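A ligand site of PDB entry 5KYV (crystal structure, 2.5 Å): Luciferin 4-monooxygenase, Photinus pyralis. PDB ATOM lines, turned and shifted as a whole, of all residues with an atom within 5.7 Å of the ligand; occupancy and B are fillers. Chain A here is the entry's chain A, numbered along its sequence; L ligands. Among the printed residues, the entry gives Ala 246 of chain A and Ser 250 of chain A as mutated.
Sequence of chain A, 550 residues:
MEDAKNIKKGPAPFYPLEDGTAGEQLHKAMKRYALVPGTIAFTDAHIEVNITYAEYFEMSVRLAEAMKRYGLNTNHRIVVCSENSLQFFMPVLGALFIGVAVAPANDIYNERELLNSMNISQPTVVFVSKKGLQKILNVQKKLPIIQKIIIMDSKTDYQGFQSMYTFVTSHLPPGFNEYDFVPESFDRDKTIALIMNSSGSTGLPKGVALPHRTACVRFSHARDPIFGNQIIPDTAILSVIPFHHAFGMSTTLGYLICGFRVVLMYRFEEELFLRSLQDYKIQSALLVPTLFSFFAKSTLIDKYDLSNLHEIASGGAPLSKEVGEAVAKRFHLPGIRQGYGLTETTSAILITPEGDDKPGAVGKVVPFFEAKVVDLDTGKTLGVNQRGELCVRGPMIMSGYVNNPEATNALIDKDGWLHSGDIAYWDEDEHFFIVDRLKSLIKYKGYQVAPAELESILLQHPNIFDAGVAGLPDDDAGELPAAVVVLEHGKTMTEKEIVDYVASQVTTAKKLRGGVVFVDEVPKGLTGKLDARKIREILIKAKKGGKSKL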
ATOM      1  N   SER A 198      23.810 -20.756  20.470  1.00  0.00           N
ATOM      2  CA  SER A 198      22.869 -21.210  21.485  1.00  0.00           C
ATOM      3  C   SER A 198      23.538 -21.923  22.672  1.00  0.00           C
ATOM      4  O   SER A 198      23.185 -21.695  23.841  1.00  0.00           O
ATOM      5  CB  SER A 198      21.843 -22.146  20.859  1.00  0.00           C
ATOM      6  OG  SER A 198      22.530 -22.953  19.938  1.00  0.00           O
ATOM      7  N   ARG A 218       9.550 -12.070  11.547  1.00  0.00           N
ATOM      8  CA  ARG A 218       9.627 -11.328  12.806  1.00  0.00           C
ATOM      9  C   ARG A 218       9.015  -9.931  12.673  1.00  0.00           C
ATOM     10  O   ARG A 218       8.321  -9.475  13.603  1.00  0.00           O
ATOM     11  CB  ARG A 218      11.076 -11.225  13.289  1.00  0.00           C
ATOM     12  CG  ARG A 218      11.247 -10.341  14.502  1.00  0.00           C
ATOM     13  CD  ARG A 218      10.416 -10.797  15.661  1.00  0.00           C
ATOM     14  NE  ARG A 218      10.390  -9.813  16.746  1.00  0.00           N
ATOM     15  CZ  ARG A 218       9.422  -9.734  17.652  1.00  0.00           C
ATOM     16  NH1 ARG A 218       8.383 -10.564  17.592  1.00  0.00           N
ATOM     17  NH2 ARG A 218       9.453  -8.827  18.606  1.00  0.00           N
ATOM     18  N   HIS A 245      21.981 -11.577  21.620  1.00  0.00           N
ATOM     19  CA  HIS A 245      21.089 -12.695  21.881  1.00  0.00           C
ATOM     20  C   HIS A 245      19.833 -12.563  21.026  1.00  0.00           C
ATOM     21  O   HIS A 245      19.448 -11.451  20.664  1.00  0.00           O
ATOM     22  CB  HIS A 245      20.721 -12.735  23.349  1.00  0.00           C
ATOM     23  CG  HIS A 245      20.062 -14.000  23.770  1.00  0.00           C
ATOM     24  ND1 HIS A 245      18.717 -14.065  24.104  1.00  0.00           N
ATOM     25  CD2 HIS A 245      20.548 -15.247  23.941  1.00  0.00           C
ATOM     26  CE1 HIS A 245      18.419 -15.301  24.460  1.00  0.00           C
ATOM     27  NE2 HIS A 245      19.512 -16.036  24.382  1.00  0.00           N
ATOM     28  N   ALA A 246      19.194 -13.682  20.706  1.00  0.00           N
ATOM     29  CA  ALA A 246      18.036 -13.650  19.800  1.00  0.00           C
ATOM     30  C   ALA A 246      16.926 -12.753  20.333  1.00  0.00           C
ATOM     31  O   ALA A 246      16.264 -12.058  19.575  1.00  0.00           O
ATOM     32  CB  ALA A 246      17.529 -15.050  19.529  1.00  0.00           C
ATOM     33  N   PHE A 247      16.728 -12.776  21.639  1.00  0.00           N
ATOM     34  CA  PHE A 247      15.810 -11.856  22.326  1.00  0.00           C
ATOM     35  C   PHE A 247      16.087 -10.387  21.934  1.00  0.00           C
ATOM     36  O   PHE A 247      15.200  -9.680  21.467  1.00  0.00           O
ATOM     37  CB  PHE A 247      15.948 -12.063  23.833  1.00  0.00           C
ATOM     38  CG  PHE A 247      14.859 -11.432  24.668  1.00  0.00           C
ATOM     39  CD1 PHE A 247      13.793 -10.750  24.086  1.00  0.00           C
ATOM     40  CD2 PHE A 247      14.909 -11.526  26.046  1.00  0.00           C
ATOM     41  CE1 PHE A 247      12.812 -10.180  24.879  1.00  0.00           C
ATOM     42  CE2 PHE A 247      13.942 -10.951  26.838  1.00  0.00           C
ATOM     43  CZ  PHE A 247      12.890 -10.288  26.258  1.00  0.00           C
ATOM     44  N   SER A 250      16.120  -9.651  17.855  1.00  0.00           N
ATOM     45  CA  SER A 250      14.846  -9.706  17.153  1.00  0.00           C
ATOM     46  C   SER A 250      13.884  -8.614  17.623  1.00  0.00           C
ATOM     47  O   SER A 250      13.094  -8.119  16.828  1.00  0.00           O
ATOM     48  CB  SER A 250      14.201 -11.082  17.305  1.00  0.00           C
ATOM     49  OG  SER A 250      13.803 -11.312  18.641  1.00  0.00           O
ATOM     50  N   THR A 251      13.949  -8.231  18.888  1.00  0.00           N
ATOM     51  CA  THR A 251      13.138  -7.101  19.344  1.00  0.00           C
ATOM     52  C   THR A 251      13.647  -5.753  18.822  1.00  0.00           C
ATOM     53  O   THR A 251      12.857  -4.900  18.405  1.00  0.00           O
ATOM     54  CB  THR A 251      13.084  -7.029  20.868  1.00  0.00           C
ATOM     55  OG1 THR A 251      14.398  -7.160  21.401  1.00  0.00           O
ATOM     56  CG2 THR A 251      12.213  -8.147  21.411  1.00  0.00           C
ATOM     57  N   LEU A 286      11.593  -3.876  28.159  1.00  0.00           N
ATOM     58  CA  LEU A 286      12.027  -5.279  28.128  1.00  0.00           C
ATOM     59  C   LEU A 286      12.849  -5.677  29.337  1.00  0.00           C
ATOM     60  O   LEU A 286      13.842  -5.026  29.656  1.00  0.00           O
ATOM     61  CB  LEU A 286      12.870  -5.545  26.888  1.00  0.00           C
ATOM     62  CG  LEU A 286      12.121  -5.736  25.569  1.00  0.00           C
ATOM     63  CD1 LEU A 286      13.088  -6.197  24.501  1.00  0.00           C
ATOM     64  CD2 LEU A 286      11.034  -6.748  25.798  1.00  0.00           C
ATOM     65  N   ALA A 313       7.577  -6.286  29.294  1.00  0.00           N
ATOM     66  CA  ALA A 313       7.646  -7.598  28.681  1.00  0.00           C
ATOM     67  C   ALA A 313       8.841  -8.412  29.175  1.00  0.00           C
ATOM     68  O   ALA A 313       9.966  -7.923  29.235  1.00  0.00           O
ATOM     69  CB  ALA A 313       7.686  -7.455  27.136  1.00  0.00           C
ATOM     70  N   SER A 314       8.603  -9.675  29.509  1.00  0.00           N
ATOM     71  CA  SER A 314       9.681 -10.536  29.963  1.00  0.00           C
ATOM     72  C   SER A 314       9.830 -11.694  28.992  1.00  0.00           C
ATOM     73  O   SER A 314       8.918 -11.972  28.229  1.00  0.00           O
ATOM     74  CB  SER A 314       9.395 -11.023  31.392  1.00  0.00           C
ATOM     75  OG  SER A 314      10.505 -11.711  31.941  1.00  0.00           O
ATOM     76  N   GLY A 315      10.982 -12.350  29.008  1.00  0.00           N
ATOM     77  CA  GLY A 315      11.235 -13.486  28.136  1.00  0.00           C
ATOM     78  C   GLY A 315      12.541 -14.168  28.514  1.00  0.00           C
ATOM     79  O   GLY A 315      13.286 -13.656  29.351  1.00  0.00           O
ATOM     80  N   GLY A 316      12.821 -15.328  27.907  1.00  0.00           N
ATOM     81  CA  GLY A 316      14.098 -16.011  28.110  1.00  0.00           C
ATOM     82  C   GLY A 316      14.192 -16.982  29.281  1.00  0.00           C
ATOM     83  O   GLY A 316      15.112 -17.790  29.361  1.00  0.00           O
ATOM     84  N   ALA A 317      13.239 -16.915  30.212  1.00  0.00           N
ATOM     85  CA  ALA A 317      13.330 -17.720  31.421  1.00  0.00           C
ATOM     86  C   ALA A 317      12.000 -17.694  32.130  1.00  0.00           C
ATOM     87  O   ALA A 317      11.214 -16.785  31.910  1.00  0.00           O
ATOM     88  CB  ALA A 317      14.455 -17.217  32.359  1.00  0.00           C
ATOM     89  N   PRO A 318      11.725 -18.711  32.947  1.00  0.00           N
ATOM     90  CA  PRO A 318      10.466 -18.741  33.698  1.00  0.00           C
ATOM     91  C   PRO A 318      10.313 -17.529  34.622  1.00  0.00           C
ATOM     92  O   PRO A 318      11.212 -17.174  35.378  1.00  0.00           O
ATOM     93  CB  PRO A 318      10.552 -20.045  34.500  1.00  0.00           C
ATOM     94  CG  PRO A 318      11.933 -20.577  34.286  1.00  0.00           C
ATOM     95  CD  PRO A 318      12.442 -20.003  33.011  1.00  0.00           C
ATOM     96  N   LEU A 319       9.150 -16.888  34.529  1.00  0.00           N
ATOM     97  CA  LEU A 319       8.820 -15.791  35.397  1.00  0.00           C
ATOM     98  C   LEU A 319       7.888 -16.323  36.441  1.00  0.00           C
ATOM     99  O   LEU A 319       6.851 -16.902  36.100  1.00  0.00           O
ATOM    100  CB  LEU A 319       8.167 -14.652  34.615  1.00  0.00           C
ATOM    101  CG  LEU A 319       7.693 -13.449  35.429  1.00  0.00           C
ATOM    102  CD1 LEU A 319       8.779 -12.903  36.367  1.00  0.00           C
ATOM    103  CD2 LEU A 319       7.235 -12.382  34.475  1.00  0.00           C
ATOM    104  N   ARG A 337       3.578  -8.855  30.231  1.00  0.00           N
ATOM    105  CA  ARG A 337       3.600  -9.469  28.923  1.00  0.00           C
ATOM    106  C   ARG A 337       4.762 -10.464  28.819  1.00  0.00           C
ATOM    107  O   ARG A 337       5.856 -10.228  29.336  1.00  0.00           O
ATOM    108  CB  ARG A 337       3.721  -8.419  27.830  1.00  0.00           C
ATOM    109  CG  ARG A 337       3.581  -9.001  26.419  1.00  0.00           C
ATOM    110  CD  ARG A 337       3.269  -7.927  25.444  1.00  0.00           C
ATOM    111  NE  ARG A 337       2.467  -8.434  24.345  1.00  0.00           N
ATOM    112  CZ  ARG A 337       2.255  -7.773  23.209  1.00  0.00           C
ATOM    113  NH1 ARG A 337       2.818  -6.577  23.025  1.00  0.00           N
ATOM    114  NH2 ARG A 337       1.513  -8.313  22.257  1.00  0.00           N
ATOM    115  N   GLN A 338       4.538 -11.578  28.138  1.00  0.00           N
ATOM    116  CA  GLN A 338       5.530 -12.621  28.102  1.00  0.00           C
ATOM    117  C   GLN A 338       5.823 -13.040  26.690  1.00  0.00           C
ATOM    118  O   GLN A 338       4.959 -12.950  25.818  1.00  0.00           O
ATOM    119  CB  GLN A 338       5.057 -13.799  28.930  1.00  0.00           C
ATOM    120  CG  GLN A 338       6.127 -14.799  29.218  1.00  0.00           C
ATOM    121  CD  GLN A 338       6.686 -14.646  30.603  1.00  0.00           C
ATOM    122  OE1 GLN A 338       6.219 -13.827  31.380  1.00  0.00           O
ATOM    123  NE2 GLN A 338       7.679 -15.464  30.929  1.00  0.00           N
ATOM    124  N   GLY A 339       7.044 -13.496  26.449  1.00  0.00           N
ATOM    125  CA  GLY A 339       7.367 -14.077  25.165  1.00  0.00           C
ATOM    126  C   GLY A 339       8.206 -15.312  25.398  1.00  0.00           C
ATOM    127  O   GLY A 339       9.100 -15.289  26.242  1.00  0.00           O
ATOM    128  N   TYR A 340       7.917 -16.401  24.696  1.00  0.00           N
ATOM    129  CA  TYR A 340       8.753 -17.592  24.804  1.00  0.00           C
ATOM    130  C   TYR A 340       9.351 -17.870  23.447  1.00  0.00           C
ATOM    131  O   TYR A 340       8.639 -17.906  22.451  1.00  0.00           O
ATOM    132  CB  TYR A 340       7.954 -18.790  25.329  1.00  0.00           C
ATOM    133  CG  TYR A 340       8.542 -20.171  25.023  1.00  0.00           C
ATOM    134  CD1 TYR A 340       8.386 -20.758  23.763  1.00  0.00           C
ATOM    135  CD2 TYR A 340       9.226 -20.891  26.002  1.00  0.00           C
ATOM    136  CE1 TYR A 340       8.918 -21.999  23.479  1.00  0.00           C
ATOM    137  CE2 TYR A 340       9.749 -22.143  25.738  1.00  0.00           C
ATOM    138  CZ  TYR A 340       9.593 -22.694  24.467  1.00  0.00           C
ATOM    139  OH  TYR A 340      10.124 -23.933  24.173  1.00  0.00           O
ATOM    140  N   GLY A 341      10.663 -18.067  23.418  1.00  0.00           N
ATOM    141  CA  GLY A 341      11.361 -18.350  22.186  1.00  0.00           C
ATOM    142  C   GLY A 341      12.647 -19.148  22.365  1.00  0.00           C
ATOM    143  O   GLY A 341      13.062 -19.465  23.468  1.00  0.00           O
ATOM    144  N   LEU A 342      13.255 -19.481  21.235  1.00  0.00           N
ATOM    145  CA  LEU A 342      14.543 -20.145  21.218  1.00  0.00           C
ATOM    146  C   LEU A 342      15.377 -19.457  20.156  1.00  0.00           C
ATOM    147  O   LEU A 342      14.834 -18.933  19.173  1.00  0.00           O
ATOM    148  CB  LEU A 342      14.406 -21.639  20.909  1.00  0.00           C
ATOM    149  CG  LEU A 342      13.826 -22.614  21.948  1.00  0.00           C
ATOM    150  CD1 LEU A 342      12.297 -22.650  21.928  1.00  0.00           C
ATOM    151  CD2 LEU A 342      14.410 -24.003  21.705  1.00  0.00           C
ATOM    152  N   THR A 343      16.686 -19.447  20.336  1.00  0.00           N
ATOM    153  CA  THR A 343      17.564 -18.881  19.325  1.00  0.00           C
ATOM    154  C   THR A 343      17.249 -19.506  17.963  1.00  0.00           C
ATOM    155  O   THR A 343      17.354 -18.844  16.934  1.00  0.00           O
ATOM    156  CB  THR A 343      19.036 -19.111  19.687  1.00  0.00           C
ATOM    157  OG1 THR A 343      19.301 -18.576  20.992  1.00  0.00           O
ATOM    158  CG2 THR A 343      19.953 -18.471  18.656  1.00  0.00           C
ATOM    159  N   GLU A 344      16.835 -20.766  17.998  1.00  0.00           N
ATOM    160  CA  GLU A 344      16.524 -21.519  16.780  1.00  0.00           C
ATOM    161  C   GLU A 344      15.144 -21.221  16.203  1.00  0.00           C
ATOM    162  O   GLU A 344      14.829 -21.709  15.115  1.00  0.00           O
ATOM    163  CB  GLU A 344      16.646 -23.003  17.043  1.00  0.00           C
ATOM    164  CG  GLU A 344      18.056 -23.469  17.309  1.00  0.00           C
ATOM    165  CD  GLU A 344      18.383 -23.482  18.774  1.00  0.00           C
ATOM    166  OE1 GLU A 344      17.787 -22.672  19.526  1.00  0.00           O
ATOM    167  OE2 GLU A 344      19.248 -24.294  19.185  1.00  0.00           O
ATOM    168  N   THR A 345      14.324 -20.458  16.908  1.00  0.00           N
ATOM    169  CA  THR A 345      13.061 -20.018  16.345  1.00  0.00           C
ATOM    170  C   THR A 345      13.103 -18.528  16.078  1.00  0.00           C
ATOM    171  O   THR A 345      12.067 -17.880  15.884  1.00  0.00           O
ATOM    172  CB  THR A 345      11.902 -20.301  17.278  1.00  0.00           C
ATOM    173  OG1 THR A 345      11.998 -19.446  18.415  1.00  0.00           O
ATOM    174  CG2 THR A 345      11.918 -21.754  17.755  1.00  0.00           C
ATOM    175  N   THR A 346      14.315 -17.976  16.104  1.00  0.00           N
ATOM    176  CA  THR A 346      14.563 -16.548  15.847  1.00  0.00           C
ATOM    177  C   THR A 346      14.027 -15.620  16.937  1.00  0.00           C
ATOM    178  O   THR A 346      14.749 -14.796  17.474  1.00  0.00           O
ATOM    179  CB  THR A 346      13.966 -16.100  14.525  1.00  0.00           C
ATOM    180  OG1 THR A 346      14.382 -17.011  13.498  1.00  0.00           O
ATOM    181  CG2 THR A 346      14.428 -14.666  14.177  1.00  0.00           C
ATOM    182  N   SER A 347      12.743 -15.734  17.244  1.00  0.00           N
ATOM    183  CA  SER A 347      12.199 -14.884  18.282  1.00  0.00           C
ATOM    184  C   SER A 347      11.113 -15.638  19.085  1.00  0.00           C
ATOM    185  O   SER A 347      11.062 -16.858  19.048  1.00  0.00           O
ATOM    186  CB  SER A 347      11.659 -13.604  17.664  1.00  0.00           C
ATOM    187  OG  SER A 347      11.199 -12.709  18.653  1.00  0.00           O
ATOM    188  N   ALA A 348      10.284 -14.907  19.804  1.00  0.00           N
ATOM    189  CA  ALA A 348       9.201 -15.526  20.538  1.00  0.00           C
ATOM    190  C   ALA A 348       8.200 -16.133  19.563  1.00  0.00           C
ATOM    191  O   ALA A 348       7.866 -15.508  18.551  1.00  0.00           O
ATOM    192  CB  ALA A 348       8.517 -14.526  21.449  1.00  0.00           C
ATOM    193  N   ILE A 351       3.623 -15.771  22.555  1.00  0.00           N
ATOM    194  CA  ILE A 351       3.578 -14.391  23.022  1.00  0.00           C
ATOM    195  C   ILE A 351       2.227 -14.118  23.677  1.00  0.00           C
ATOM    196  O   ILE A 351       1.202 -14.626  23.215  1.00  0.00           O
ATOM    197  CB  ILE A 351       3.784 -13.406  21.859  1.00  0.00           C
ATOM    198  CG1 ILE A 351       5.154 -13.622  21.215  1.00  0.00           C
ATOM    199  CG2 ILE A 351       3.672 -11.983  22.343  1.00  0.00           C
ATOM    200  CD1 ILE A 351       5.427 -12.690  20.022  1.00  0.00           C
ATOM    201  N   VAL A 362       2.861 -18.205  29.205  1.00  0.00           N
ATOM    202  CA  VAL A 362       3.762 -17.491  28.327  1.00  0.00           C
ATOM    203  C   VAL A 362       3.066 -17.022  27.056  1.00  0.00           C
ATOM    204  O   VAL A 362       3.679 -16.432  26.177  1.00  0.00           O
ATOM    205  CB  VAL A 362       4.948 -18.358  27.934  1.00  0.00           C
ATOM    206  CG1 VAL A 362       5.834 -18.619  29.147  1.00  0.00           C
ATOM    207  CG2 VAL A 362       4.446 -19.660  27.328  1.00  0.00           C
ATOM    208  N   SER A 420      11.848 -28.668  21.458  1.00  0.00           N
ATOM    209  CA  SER A 420      12.393 -27.588  22.236  1.00  0.00           C
ATOM    210  C   SER A 420      13.218 -28.027  23.412  1.00  0.00           C
ATOM    211  O   SER A 420      13.974 -27.226  23.977  1.00  0.00           O
ATOM    212  CB  SER A 420      11.262 -26.738  22.771  1.00  0.00           C
ATOM    213  OG  SER A 420      10.585 -27.464  23.775  1.00  0.00           O
ATOM    214  N   ASP A 422      11.745 -28.431  26.065  1.00  0.00           N
ATOM    215  CA  ASP A 422      10.940 -27.901  27.169  1.00  0.00           C
ATOM    216  C   ASP A 422       9.665 -28.718  27.433  1.00  0.00           C
ATOM    217  O   ASP A 422       8.984 -29.168  26.503  1.00  0.00           O
ATOM    218  CB  ASP A 422      10.549 -26.448  26.906  1.00  0.00           C
ATOM    219  CG  ASP A 422      11.741 -25.543  26.782  1.00  0.00           C
ATOM    220  OD1 ASP A 422      12.581 -25.549  27.704  1.00  0.00           O
ATOM    221  OD2 ASP A 422      11.839 -24.834  25.768  1.00  0.00           O
ATOM    222  N   ILE A 434       4.807 -23.135  30.494  1.00  0.00           N
ATOM    223  CA  ILE A 434       6.111 -23.775  30.555  1.00  0.00           C
ATOM    224  C   ILE A 434       6.385 -24.329  31.952  1.00  0.00           C
ATOM    225  O   ILE A 434       6.285 -23.611  32.947  1.00  0.00           O
ATOM    226  CB  ILE A 434       7.201 -22.784  30.170  1.00  0.00           C
ATOM    227  CG1 ILE A 434       6.930 -22.286  28.755  1.00  0.00           C
ATOM    228  CG2 ILE A 434       8.563 -23.449  30.199  1.00  0.00           C
ATOM    229  CD1 ILE A 434       6.886 -23.419  27.697  1.00  0.00           C
ATOM    230  N   ARG A 437      12.771 -26.865  31.695  1.00  0.00           N
ATOM    231  CA  ARG A 437      13.565 -27.700  30.816  1.00  0.00           C
ATOM    232  C   ARG A 437      13.324 -29.134  31.231  1.00  0.00           C
ATOM    233  O   ARG A 437      13.305 -29.436  32.427  1.00  0.00           O
ATOM    234  CB  ARG A 437      15.048 -27.353  30.892  1.00  0.00           C
ATOM    235  CG  ARG A 437      15.386 -25.958  30.413  1.00  0.00           C
ATOM    236  CD  ARG A 437      15.352 -25.931  28.905  1.00  0.00           C
ATOM    237  NE  ARG A 437      16.468 -26.631  28.267  1.00  0.00           N
ATOM    238  CZ  ARG A 437      16.457 -27.019  26.998  1.00  0.00           C
ATOM    239  NH1 ARG A 437      15.369 -26.811  26.254  1.00  0.00           N
ATOM    240  NH2 ARG A 437      17.516 -27.650  26.468  1.00  0.00           N
ATOM    241  N   LEU A 526      23.272 -16.299  30.799  1.00  0.00           N
ATOM    242  CA  LEU A 526      22.622 -15.647  29.644  1.00  0.00           C
ATOM    243  C   LEU A 526      21.644 -14.543  30.024  1.00  0.00           C
ATOM    244  O   LEU A 526      21.991 -13.603  30.754  1.00  0.00           O
ATOM    245  CB  LEU A 526      21.879 -16.691  28.783  1.00  0.00           C
ATOM    246  CG  LEU A 526      22.639 -17.528  27.751  1.00  0.00           C
ATOM    247  CD1 LEU A 526      21.675 -18.059  26.683  1.00  0.00           C
ATOM    248  CD2 LEU A 526      23.731 -16.714  27.113  1.00  0.00           C
ATOM    249  N   THR A 527      20.423 -14.680  29.510  1.00  0.00           N
ATOM    250  CA  THR A 527      19.319 -13.752  29.763  1.00  0.00           C
ATOM    251  C   THR A 527      18.619 -14.104  31.060  1.00  0.00           C
ATOM    252  O   THR A 527      17.415 -14.350  31.086  1.00  0.00           O
ATOM    253  CB  THR A 527      18.268 -13.768  28.606  1.00  0.00           C
ATOM    254  OG1 THR A 527      17.947 -15.125  28.251  1.00  0.00           O
ATOM    255  CG2 THR A 527      18.782 -13.032  27.365  1.00  0.00           C
HETATM  256  O1  LIG L   1      15.608 -17.473  25.268  1.00  0.00           O
HETATM  257  C1  LIG L   1      15.761 -17.456  24.066  1.00  0.00           C
HETATM  258  C2  LIG L   1      14.987 -16.572  23.207  1.00  0.00           C
HETATM  259  N1  LIG L   1      14.074 -15.757  23.682  1.00  0.00           N
HETATM  260  C3  LIG L   1      15.250 -16.598  21.851  1.00  0.00           C
HETATM  261  S1  LIG L   1      14.136 -15.421  21.250  1.00  0.00           S
HETATM  262  C4  LIG L   1      13.431 -14.999  22.832  1.00  0.00           C
HETATM  263  C5  LIG L   1      12.382 -14.018  23.077  1.00  0.00           C
HETATM  264  S2  LIG L   1      11.539 -13.697  24.598  1.00  0.00           S
HETATM  265  C6  LIG L   1      10.504 -12.417  23.955  1.00  0.00           C
HETATM  266  C7  LIG L   1       9.547 -11.624  24.498  1.00  0.00           C
HETATM  267  C8  LIG L   1       9.018 -10.618  23.713  1.00  0.00           C
HETATM  268  O2  LIG L   1       8.115  -9.748  24.244  1.00  0.00           O
HETATM  269  C9  LIG L   1      10.913 -12.325  22.598  1.00  0.00           C
HETATM  270  N2  LIG L   1      11.872 -13.169  22.222  1.00  0.00           N
HETATM  271  C10 LIG L   1      10.261 -11.364  21.787  1.00  0.00           C
HETATM  272  C11 LIG L   1       9.410 -10.496  22.369  1.00  0.00           C
HETATM  273  N3  LIG L   1      16.620 -18.247  23.408  1.00  0.00           N
HETATM  274  S3  LIG L   1      17.568 -19.345  24.187  1.00  0.00           S
HETATM  275  O3  LIG L   1      18.648 -18.591  24.717  1.00  0.00           O
HETATM  276  O4  LIG L   1      17.665 -20.390  23.250  1.00  0.00           O
HETATM  277  O5  LIG L   1      16.857 -19.861  25.408  1.00  0.00           O
HETATM  278  C12 LIG L   1      15.900 -20.838  25.020  1.00  0.00           C
HETATM  279  C13 LIG L   1      15.236 -21.401  26.302  1.00  0.00           C
HETATM  280  C14 LIG L   1      13.894 -22.123  26.065  1.00  0.00           C
HETATM  281  O6  LIG L   1      14.044 -23.478  25.666  1.00  0.00           O
HETATM  282  C15 LIG L   1      13.246 -22.086  27.461  1.00  0.00           C
HETATM  283  O7  LIG L   1      13.848 -23.108  28.245  1.00  0.00           O
HETATM  284  C16 LIG L   1      13.732 -20.720  28.004  1.00  0.00           C
HETATM  285  O8  LIG L   1      14.856 -20.304  27.192  1.00  0.00           O
HETATM  286  N4  LIG L   1      12.694 -19.685  27.952  1.00  0.00           N
HETATM  287  C17 LIG L   1      11.607 -19.520  28.772  1.00  0.00           C
HETATM  288  N5  LIG L   1      11.114 -20.167  29.830  1.00  0.00           N
HETATM  289  C18 LIG L   1      10.020 -19.747  30.437  1.00  0.00           C
HETATM  290  N6  LIG L   1       9.366 -18.659  30.035  1.00  0.00           N
HETATM  291  C19 LIG L   1      10.930 -18.366  28.319  1.00  0.00           C
HETATM  292  C20 LIG L   1       9.778 -17.949  28.992  1.00  0.00           C
HETATM  293  N7  LIG L   1       9.076 -16.836  28.586  1.00  0.00           N
HETATM  294  N8  LIG L   1      11.618 -17.920  27.255  1.00  0.00           N
HETATM  295  C21 LIG L   1      12.645 -18.689  27.033  1.00  0.00           C
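A nitrogen (N6) of the ligand lies close to the backbone carbonyl oxygen (O) of Ala 317 (3.2 Å). The backbone nitrogen of Pro 318 lies close to a nitrogen (N5) of the ligand (3.5 Å). CB of Ala 246 touches C3 of the ligand (3.6 Å). Thr 251 touches the ligand (CG2 to C11, 3.8 Å). CB of Ala 313 touches O2 of the ligand (3.7 Å). O of Ser 314 touches C7 of the ligand (3.8 Å). Gly 315 touches the ligand. Tyr 340 touches the ligand. O of Gly 341 touches C1 of the ligand, at 3.4 Å. Leu 342 touches the ligand. O of Thr 346 touches S1 of the ligand, at 3.9 Å. Ser 347 touches the ligand. Val 362 touches the ligand. Ile 434 touches the ligand (CG2 to C18, 3.99 Å). Arg 437 touches the ligand (CD to O7, 3.3 Å). Leu 526 touches the ligand (CD1 to O3, 3.6 Å). Hydrophobic or aromatic side chains that line the ligand: His 245, Ala 246, Phe 247, Ala 313, Pro 318, Tyr 340, Leu 342, Ala 348, Val 362, Ile 434 and Leu 526. Within 4 Å of the ligand: His 245, Ala 246, Phe 247, Thr 251, Ala 313, Ser 314, Gly 315, Gly 316, Ala 317, Pro 318, Gln 338, Gly 339, Tyr 340, Gly 341, Leu 342, Thr 343, Thr 346, Ser 347, Ala 348, Val 362, Asp 422, Ile 434, Arg 437 and Leu 526. Along chain A the residues within 4 Å of the ligand span positions 245 to 526.
OD2 of Asp 422 lies within hydrogen-bond range of O6 of the ligand, at 2.6 Å. O3 of the ligand sits at hydrogen-bond distance from NE2 of His 245, at 2.7 Å. A nitrogen (N7) of the ligand is in hydrogen-bond range of the backbone carbonyl oxygen (O) of Gly 339 (2.8 Å). N of Gly 316 lies within hydrogen-bond range of N8 of the ligand, at 2.9 Å. The side-chain amide nitrogen of Gln 338 sits close to a nitrogen (N7) of the ligand (3.1 Å). N of Thr 343 sits at hydrogen-bond distance from O4 of the ligand, at 3.2 Å. An oxygen (O4) of the ligand sits at hydrogen-bond distance from the side-chain hydroxyl of Thr 343, at 3.3 Å. N of Phe 247 sits close to S1 of the ligand, at 3.7 Å. The backbone NH (N) of Ala 348 lies within hydrogen-bond range of a nitrogen (N2) of the ligand.
OD1 of Asp 422 lies within salt-bridge range of NH1 of Arg 437 (3.4 Å). The backbone carbonyl oxygen (O) of Ser 314 sits at hydrogen-bond distance from the backbone NH (N) of Gly 339. The guanidinium group of Arg 437 lies within hydrogen-bond range of the backbone carbonyl oxygen of Ser 420 (2.7 Å). O of Leu 342 is in hydrogen-bond range of OG1 of Thr 345 (3.0 Å). The backbone carbonyl oxygen of Phe 247 lies within hydrogen-bond range of the side-chain hydroxyl of Thr 251. The side-chain hydroxyl (OG) of Ser 250 lies within hydrogen-bond range of the side-chain hydroxyl (OG) of Ser 347 (3.0 Å). O of Ser 347 is in hydrogen-bond range of OG1 of Thr 345 (2.8 Å). The backbone carbonyl oxygen (O) of Ala 246 is in hydrogen-bond range of the side-chain hydroxyl (OG) of Ser 250, 2.7 Å away.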
